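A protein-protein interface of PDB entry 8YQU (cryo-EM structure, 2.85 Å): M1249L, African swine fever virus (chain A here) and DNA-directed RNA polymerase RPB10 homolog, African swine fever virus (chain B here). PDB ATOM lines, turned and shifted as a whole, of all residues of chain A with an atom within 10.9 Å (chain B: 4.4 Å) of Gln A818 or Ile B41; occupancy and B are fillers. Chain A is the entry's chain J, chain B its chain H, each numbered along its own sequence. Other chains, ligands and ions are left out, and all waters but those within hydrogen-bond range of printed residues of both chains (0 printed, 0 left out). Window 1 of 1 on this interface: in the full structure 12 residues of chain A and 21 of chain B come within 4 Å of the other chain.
O of Ala A814 sits at hydrogen-bond distance from NE2 of Gln A818 (3.0 Å).
Among the printed residues, pairs that only touch across the chains: Glu A811 with Pro B38 (3.5 Å), Ala A814 with Pro B38 (3.9 Å), Leu A815 with Met B33 (3.8 Å), Leu A815 with Pro B38 (3.4 Å), Gln A818 with Ile B29 (3.3 Å), Gln A818 with Ile B41 (3.9 Å), Gln A818 with Pro B42 (3.5 Å), Gln A819 with Arg B25 (3.9 Å), Phe A821 with Ile B41 (3.7 Å), Phe A821 with Pro B42 (3.7 Å), Phe A821 with Leu B47 (3.8 Å) and Tyr A822 with Leu B47 (3.8 Å).
The backbone carbonyl oxygen (O) of Pro B38 lies within hydrogen-bond range of the side-chain amide nitrogen (NE2) of Gln A818 (3.3 Å).
The backbone carbonyl oxygen (O) of Leu B47 lies within hydrogen-bond range of the backbone NH (N) of Asn A823, at 3.2 Å.
Printed residues of chain B that touch a printed residue of chain A: Arg B25, Ile B29, Met B33, Pro B38, Ile B41, Pro B42 and Leu B47.
Hydrophobic or aromatic side chains of chain B that line the printed part of chain A: Ile B29, Met B33, Pro B38, Ile B41, Pro B42 and Leu B47.
Hydrophobic or aromatic side chains of chain A that line the printed part of chain B: Leu A815 and Phe A821.
Along chain A the printed residues that touch a printed residue of chain B span positions 811 to 823.
Among the printed residues, no Asp or Glu carboxylate lies within 4 Å of a Lys or Arg side-chain nitrogen of the other chain.
Printed residues of chain B within 4 Å of Glu A811: Pro B38.
Printed residues of chain B within 4 Å of Ala A814: Pro B38.
Of chain B, only Ile B29, Pro B38, Ile B41 and Pro B42 come within 4 Å of Gln A818.
Of the printed residues of chain B, Tyr A822 touches Leu B47.
Of the printed residues of chain B, Asn A823 touches Leu B47.
Of the printed residues of chain A, Met B33 touches Leu A815.
Printed residues of chain A within 4 Å of Ile B41: Gln A818 and Phe A821.
Pro B42 touches two residues of chain A.
No residue of chain A comes within 4 Å of Asp B44.
The nearest residue of chain A that does not touch Ile B41 is Gly A820 (4.9 Å).
The nearest printed residue of chain B that does not touch Leu A815 is Ile B29 (4.4 Å).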
ATOM      1  N   GLY A 810       6.424  -6.213  17.874  1.00  0.00           N
ATOM      2  CA  GLY A 810       7.146  -7.433  18.181  1.00  0.00           C
ATOM      3  C   GLY A 810       6.325  -8.420  18.981  1.00  0.00           C
ATOM      4  O   GLY A 810       6.473  -9.631  18.810  1.00  0.00           O
ATOM      5  N   GLU A 811       5.465  -7.924  19.873  1.00  0.00           N
ATOM      6  CA  GLU A 811       4.525  -8.812  20.551  1.00  0.00           C
ATOM      7  C   GLU A 811       3.613  -9.502  19.545  1.00  0.00           C
ATOM      8  O   GLU A 811       3.386 -10.717  19.626  1.00  0.00           O
ATOM      9  CB  GLU A 811       3.695  -8.034  21.571  1.00  0.00           C
ATOM     10  CG  GLU A 811       4.480  -7.507  22.757  1.00  0.00           C
ATOM     11  CD  GLU A 811       3.606  -6.742  23.732  1.00  0.00           C
ATOM     12  OE1 GLU A 811       2.419  -6.519  23.418  1.00  0.00           O
ATOM     13  OE2 GLU A 811       4.106  -6.363  24.812  1.00  0.00           O
ATOM     14  N   GLN A 812       3.093  -8.742  18.578  1.00  0.00           N
ATOM     15  CA  GLN A 812       2.270  -9.356  17.536  1.00  0.00           C
ATOM     16  C   GLN A 812       3.064 -10.385  16.732  1.00  0.00           C
ATOM     17  O   GLN A 812       2.569 -11.485  16.442  1.00  0.00           O
ATOM     18  CB  GLN A 812       1.695  -8.283  16.613  1.00  0.00           C
ATOM     19  CG  GLN A 812       0.675  -7.374  17.272  1.00  0.00           C
ATOM     20  CD  GLN A 812      -0.065  -6.511  16.270  1.00  0.00           C
ATOM     21  OE1 GLN A 812      -0.050  -6.784  15.070  1.00  0.00           O
ATOM     22  NE2 GLN A 812      -0.718  -5.464  16.758  1.00  0.00           N
ATOM     23  N   LYS A 813       4.301 -10.046  16.367  1.00  0.00           N
ATOM     24  CA  LYS A 813       5.122 -10.955  15.572  1.00  0.00           C
ATOM     25  C   LYS A 813       5.446 -12.230  16.344  1.00  0.00           C
ATOM     26  O   LYS A 813       5.491 -13.321  15.764  1.00  0.00           O
ATOM     27  CB  LYS A 813       6.402 -10.249  15.131  1.00  0.00           C
ATOM     28  CG  LYS A 813       7.281 -11.068  14.204  1.00  0.00           C
ATOM     29  CD  LYS A 813       8.486 -10.268  13.745  1.00  0.00           C
ATOM     30  CE  LYS A 813       9.374 -11.085  12.824  1.00  0.00           C
ATOM     31  NZ  LYS A 813      10.557 -10.304  12.373  1.00  0.00           N
ATOM     32  N   ALA A 814       5.681 -12.109  17.652  1.00  0.00           N
ATOM     33  CA  ALA A 814       5.891 -13.287  18.485  1.00  0.00           C
ATOM     34  C   ALA A 814       4.622 -14.115  18.602  1.00  0.00           C
ATOM     35  O   ALA A 814       4.693 -15.343  18.724  1.00  0.00           O
ATOM     36  CB  ALA A 814       6.389 -12.875  19.869  1.00  0.00           C
ATOM     37  N   LEU A 815       3.456 -13.464  18.580  1.00  0.00           N
ATOM     38  CA  LEU A 815       2.208 -14.213  18.477  1.00  0.00           C
ATOM     39  C   LEU A 815       2.171 -15.018  17.187  1.00  0.00           C
ATOM     40  O   LEU A 815       1.710 -16.166  17.172  1.00  0.00           O
ATOM     41  CB  LEU A 815       1.012 -13.263  18.554  1.00  0.00           C
ATOM     42  CG  LEU A 815      -0.375 -13.830  18.236  1.00  0.00           C
ATOM     43  CD1 LEU A 815      -0.666 -15.082  19.054  1.00  0.00           C
ATOM     44  CD2 LEU A 815      -1.448 -12.777  18.462  1.00  0.00           C
ATOM     45  N   LEU A 816       2.663 -14.434  16.092  1.00  0.00           N
ATOM     46  CA  LEU A 816       2.715 -15.162  14.829  1.00  0.00           C
ATOM     47  C   LEU A 816       3.740 -16.292  14.834  1.00  0.00           C
ATOM     48  O   LEU A 816       3.732 -17.118  13.916  1.00  0.00           O
ATOM     49  CB  LEU A 816       3.018 -14.203  13.679  1.00  0.00           C
ATOM     50  CG  LEU A 816       1.891 -13.251  13.276  1.00  0.00           C
ATOM     51  CD1 LEU A 816       2.348 -12.319  12.165  1.00  0.00           C
ATOM     52  CD2 LEU A 816       0.659 -14.033  12.854  1.00  0.00           C
ATOM     53  N   ALA A 817       4.613 -16.359  15.839  1.00  0.00           N
ATOM     54  CA  ALA A 817       5.750 -17.276  15.843  1.00  0.00           C
ATOM     55  C   ALA A 817       5.657 -18.329  16.945  1.00  0.00           C
ATOM     56  O   ALA A 817       6.653 -18.647  17.599  1.00  0.00           O
ATOM     57  CB  ALA A 817       7.058 -16.502  15.973  1.00  0.00           C
ATOM     58  N   GLN A 818       4.471 -18.890  17.165  1.00  0.00           N
ATOM     59  CA  GLN A 818       4.260 -19.893  18.203  1.00  0.00           C
ATOM     60  C   GLN A 818       3.926 -21.234  17.563  1.00  0.00           C
ATOM     61  O   GLN A 818       2.980 -21.331  16.775  1.00  0.00           O
ATOM     62  CB  GLN A 818       3.148 -19.464  19.159  1.00  0.00           C
ATOM     63  CG  GLN A 818       3.471 -18.217  19.966  1.00  0.00           C
ATOM     64  CD  GLN A 818       4.759 -18.351  20.758  1.00  0.00           C
ATOM     65  OE1 GLN A 818       5.066 -19.418  21.291  1.00  0.00           O
ATOM     66  NE2 GLN A 818       5.518 -17.266  20.839  1.00  0.00           N
ATOM     67  N   GLN A 819       4.704 -22.265  17.906  1.00  0.00           N
ATOM     68  CA  GLN A 819       4.419 -23.615  17.436  1.00  0.00           C
ATOM     69  C   GLN A 819       3.261 -24.258  18.188  1.00  0.00           C
ATOM     70  O   GLN A 819       2.668 -25.218  17.684  1.00  0.00           O
ATOM     71  CB  GLN A 819       5.659 -24.501  17.574  1.00  0.00           C
ATOM     72  CG  GLN A 819       6.978 -23.806  17.292  1.00  0.00           C
ATOM     73  CD  GLN A 819       7.192 -23.534  15.820  1.00  0.00           C
ATOM     74  OE1 GLN A 819       6.888 -24.372  14.973  1.00  0.00           O
ATOM     75  NE2 GLN A 819       7.723 -22.358  15.506  1.00  0.00           N
ATOM     76  N   GLY A 820       2.933 -23.758  19.369  1.00  0.00           N
ATOM     77  CA  GLY A 820       1.937 -24.358  20.229  1.00  0.00           C
ATOM     78  C   GLY A 820       2.560 -24.960  21.478  1.00  0.00           C
ATOM     79  O   GLY A 820       3.779 -25.079  21.616  1.00  0.00           O
ATOM     80  N   PHE A 821       1.684 -25.342  22.404  1.00  0.00           N
ATOM     81  CA  PHE A 821       2.120 -25.917  23.667  1.00  0.00           C
ATOM     82  C   PHE A 821       1.025 -26.824  24.205  1.00  0.00           C
ATOM     83  O   PHE A 821      -0.165 -26.572  24.003  1.00  0.00           O
ATOM     84  CB  PHE A 821       2.464 -24.826  24.688  1.00  0.00           C
ATOM     85  CG  PHE A 821       3.047 -25.354  25.965  1.00  0.00           C
ATOM     86  CD1 PHE A 821       4.173 -26.158  25.945  1.00  0.00           C
ATOM     87  CD2 PHE A 821       2.474 -25.043  27.185  1.00  0.00           C
ATOM     88  CE1 PHE A 821       4.712 -26.646  27.115  1.00  0.00           C
ATOM     89  CE2 PHE A 821       3.012 -25.528  28.361  1.00  0.00           C
ATOM     90  CZ  PHE A 821       4.132 -26.330  28.325  1.00  0.00           C
ATOM     91  N   TYR A 822       1.440 -27.887  24.891  1.00  0.00           N
ATOM     92  CA  TYR A 822       0.513 -28.862  25.440  1.00  0.00           C
ATOM     93  C   TYR A 822       0.965 -29.271  26.833  1.00  0.00           C
ATOM     94  O   TYR A 822       2.161 -29.318  27.128  1.00  0.00           O
ATOM     95  CB  TYR A 822       0.407 -30.100  24.544  1.00  0.00           C
ATOM     96  CG  TYR A 822      -0.672 -31.075  24.954  1.00  0.00           C
ATOM     97  CD1 TYR A 822      -2.007 -30.822  24.675  1.00  0.00           C
ATOM     98  CD2 TYR A 822      -0.355 -32.255  25.613  1.00  0.00           C
ATOM     99  CE1 TYR A 822      -2.995 -31.712  25.045  1.00  0.00           C
ATOM    100  CE2 TYR A 822      -1.335 -33.151  25.986  1.00  0.00           C
ATOM    101  CZ  TYR A 822      -2.653 -32.874  25.700  1.00  0.00           C
ATOM    102  OH  TYR A 822      -3.633 -33.765  26.071  1.00  0.00           O
ATOM    103  N   ASN A 823      -0.011 -29.570  27.687  1.00  0.00           N
ATOM    104  CA  ASN A 823       0.239 -30.048  29.041  1.00  0.00           C
ATOM    105  C   ASN A 823      -0.562 -31.322  29.254  1.00  0.00           C
ATOM    106  O   ASN A 823      -1.777 -31.335  29.035  1.00  0.00           O
ATOM    107  CB  ASN A 823      -0.145 -28.991  30.078  1.00  0.00           C
ATOM    108  CG  ASN A 823       0.753 -27.776  30.026  1.00  0.00           C
ATOM    109  OD1 ASN A 823       0.340 -26.707  29.579  1.00  0.00           O
ATOM    110  ND2 ASN A 823       1.988 -27.932  30.485  1.00  0.00           N
ATOM    111  N   ARG B  25      -3.070 -22.336  11.641  1.00  0.00           N
ATOM    112  CA  ARG B  25      -2.655 -22.659  13.003  1.00  0.00           C
ATOM    113  C   ARG B  25      -2.736 -21.432  13.896  1.00  0.00           C
ATOM    114  O   ARG B  25      -3.230 -21.502  15.028  1.00  0.00           O
ATOM    115  CB  ARG B  25      -1.236 -23.229  13.002  1.00  0.00           C
ATOM    116  CG  ARG B  25      -0.649 -23.419  14.389  1.00  0.00           C
ATOM    117  CD  ARG B  25       0.664 -24.177  14.341  1.00  0.00           C
ATOM    118  NE  ARG B  25       1.686 -23.452  13.597  1.00  0.00           N
ATOM    119  CZ  ARG B  25       2.898 -23.925  13.338  1.00  0.00           C
ATOM    120  NH1 ARG B  25       3.279 -25.119  13.761  1.00  0.00           N
ATOM    121  NH2 ARG B  25       3.749 -23.180  12.639  1.00  0.00           N
ATOM    122  N   ILE B  29      -4.480 -20.985  17.562  1.00  0.00           N
ATOM    123  CA  ILE B  29      -3.809 -20.528  18.773  1.00  0.00           C
ATOM    124  C   ILE B  29      -4.539 -19.325  19.351  1.00  0.00           C
ATOM    125  O   ILE B  29      -4.772 -19.247  20.565  1.00  0.00           O
ATOM    126  CB  ILE B  29      -2.329 -20.220  18.483  1.00  0.00           C
ATOM    127  CG1 ILE B  29      -1.524 -21.519  18.438  1.00  0.00           C
ATOM    128  CG2 ILE B  29      -1.758 -19.279  19.530  1.00  0.00           C
ATOM    129  CD1 ILE B  29      -0.072 -21.324  18.085  1.00  0.00           C
ATOM    130  N   MET B  33      -5.465 -19.164  23.052  1.00  0.00           N
ATOM    131  CA  MET B  33      -4.384 -18.454  23.727  1.00  0.00           C
ATOM    132  C   MET B  33      -4.766 -18.041  25.143  1.00  0.00           C
ATOM    133  O   MET B  33      -4.268 -18.617  26.114  1.00  0.00           O
ATOM    134  CB  MET B  33      -3.990 -17.224  22.902  1.00  0.00           C
ATOM    135  CG  MET B  33      -2.852 -16.403  23.468  1.00  0.00           C
ATOM    136  SD  MET B  33      -2.432 -15.015  22.399  1.00  0.00           S
ATOM    137  CE  MET B  33      -3.852 -13.953  22.647  1.00  0.00           C
ATOM    138  N   LEU B  37       0.304 -13.302  27.342  1.00  0.00           N
ATOM    139  CA  LEU B  37       1.201 -12.694  26.375  1.00  0.00           C
ATOM    140  C   LEU B  37       1.698 -13.748  25.387  1.00  0.00           C
ATOM    141  O   LEU B  37       1.874 -14.916  25.748  1.00  0.00           O
ATOM    142  CB  LEU B  37       2.384 -12.036  27.080  1.00  0.00           C
ATOM    143  CG  LEU B  37       2.075 -10.737  27.822  1.00  0.00           C
ATOM    144  CD1 LEU B  37       3.361 -10.041  28.234  1.00  0.00           C
ATOM    145  CD2 LEU B  37       1.215  -9.822  26.966  1.00  0.00           C
ATOM    146  N   PRO B  38       1.911 -13.363  24.127  1.00  0.00           N
ATOM    147  CA  PRO B  38       2.331 -14.356  23.121  1.00  0.00           C
ATOM    148  C   PRO B  38       3.619 -15.083  23.472  1.00  0.00           C
ATOM    149  O   PRO B  38       3.663 -16.320  23.429  1.00  0.00           O
ATOM    150  CB  PRO B  38       2.479 -13.505  21.857  1.00  0.00           C
ATOM    151  CG  PRO B  38       1.530 -12.374  22.063  1.00  0.00           C
ATOM    152  CD  PRO B  38       1.635 -12.050  23.521  1.00  0.00           C
ATOM    153  N   GLN B  39       4.669 -14.350  23.846  1.00  0.00           N
ATOM    154  CA  GLN B  39       5.953 -14.981  24.125  1.00  0.00           C
ATOM    155  C   GLN B  39       5.914 -15.880  25.352  1.00  0.00           C
ATOM    156  O   GLN B  39       6.864 -16.638  25.572  1.00  0.00           O
ATOM    157  CB  GLN B  39       7.042 -13.918  24.291  1.00  0.00           C
ATOM    158  CG  GLN B  39       6.918 -13.072  25.548  1.00  0.00           C
ATOM    159  CD  GLN B  39       5.990 -11.888  25.369  1.00  0.00           C
ATOM    160  OE1 GLN B  39       5.199 -11.839  24.427  1.00  0.00           O
ATOM    161  NE2 GLN B  39       6.083 -10.922  26.276  1.00  0.00           N
ATOM    162  N   ASN B  40       4.849 -15.818  26.148  1.00  0.00           N
ATOM    163  CA  ASN B  40       4.675 -16.688  27.302  1.00  0.00           C
ATOM    164  C   ASN B  40       3.766 -17.876  27.008  1.00  0.00           C
ATOM    165  O   ASN B  40       3.365 -18.577  27.941  1.00  0.00           O
ATOM    166  CB  ASN B  40       4.124 -15.888  28.484  1.00  0.00           C
ATOM    167  CG  ASN B  40       5.105 -14.852  28.995  1.00  0.00           C
ATOM    168  OD1 ASN B  40       6.314 -15.083  29.022  1.00  0.00           O
ATOM    169  ND2 ASN B  40       4.589 -13.700  29.406  1.00  0.00           N
ATOM    170  N   ILE B  41       3.422 -18.109  25.737  1.00  0.00           N
ATOM    171  CA  ILE B  41       2.585 -19.263  25.395  1.00  0.00           C
ATOM    172  C   ILE B  41       3.219 -20.591  25.797  1.00  0.00           C
ATOM    173  O   ILE B  41       2.524 -21.419  26.409  1.00  0.00           O
ATOM    174  CB  ILE B  41       2.198 -19.216  23.904  1.00  0.00           C
ATOM    175  CG1 ILE B  41       1.134 -18.148  23.674  1.00  0.00           C
ATOM    176  CG2 ILE B  41       1.700 -20.572  23.433  1.00  0.00           C
ATOM    177  CD1 ILE B  41      -0.182 -18.492  24.311  1.00  0.00           C
ATOM    178  N   PRO B  42       4.496 -20.864  25.514  1.00  0.00           N
ATOM    179  CA  PRO B  42       5.082 -22.147  25.917  1.00  0.00           C
ATOM    180  C   PRO B  42       5.353 -22.282  27.408  1.00  0.00           C
ATOM    181  O   PRO B  42       6.038 -23.227  27.807  1.00  0.00           O
ATOM    182  CB  PRO B  42       6.399 -22.189  25.124  1.00  0.00           C
ATOM    183  CG  PRO B  42       6.720 -20.788  24.849  1.00  0.00           C
ATOM    184  CD  PRO B  42       5.421 -20.096  24.658  1.00  0.00           C
ATOM    185  N   LEU B  43       4.841 -21.369  28.237  1.00  0.00           N
ATOM    186  CA  LEU B  43       4.990 -21.454  29.683  1.00  0.00           C
ATOM    187  C   LEU B  43       3.657 -21.327  30.410  1.00  0.00           C
ATOM    188  O   LEU B  43       3.649 -21.121  31.629  1.00  0.00           O
ATOM    189  CB  LEU B  43       5.957 -20.375  30.187  1.00  0.00           C
ATOM    190  CG  LEU B  43       7.439 -20.567  29.865  1.00  0.00           C
ATOM    191  CD1 LEU B  43       8.256 -19.427  30.444  1.00  0.00           C
ATOM    192  CD2 LEU B  43       7.936 -21.902  30.393  1.00  0.00           C
ATOM    193  N   ASP B  44       2.532 -21.441  29.700  1.00  0.00           N
ATOM    194  CA  ASP B  44       1.233 -21.198  30.320  1.00  0.00           C
ATOM    195  C   ASP B  44       0.868 -22.280  31.329  1.00  0.00           C
ATOM    196  O   ASP B  44       0.166 -21.996  32.307  1.00  0.00           O
ATOM    197  CB  ASP B  44       0.151 -21.087  29.250  1.00  0.00           C
ATOM    198  CG  ASP B  44      -1.112 -20.422  29.763  1.00  0.00           C
ATOM    199  OD1 ASP B  44      -1.121 -19.972  30.927  1.00  0.00           O
ATOM    200  OD2 ASP B  44      -2.098 -20.350  29.002  1.00  0.00           O
ATOM    201  N   LEU B  47      -2.394 -24.910  28.794  1.00  0.00           N
ATOM    202  CA  LEU B  47      -2.836 -24.975  27.411  1.00  0.00           C
ATOM    203  C   LEU B  47      -2.998 -26.418  26.955  1.00  0.00           C
ATOM    204  O   LEU B  47      -2.320 -27.328  27.441  1.00  0.00           O
ATOM    205  CB  LEU B  47      -1.848 -24.250  26.499  1.00  0.00           C
ATOM    206  CG  LEU B  47      -1.769 -22.736  26.685  1.00  0.00           C
ATOM    207  CD1 LEU B  47      -0.737 -22.136  25.750  1.00  0.00           C
ATOM    208  CD2 LEU B  47      -3.131 -22.103  26.461  1.00  0.00           C
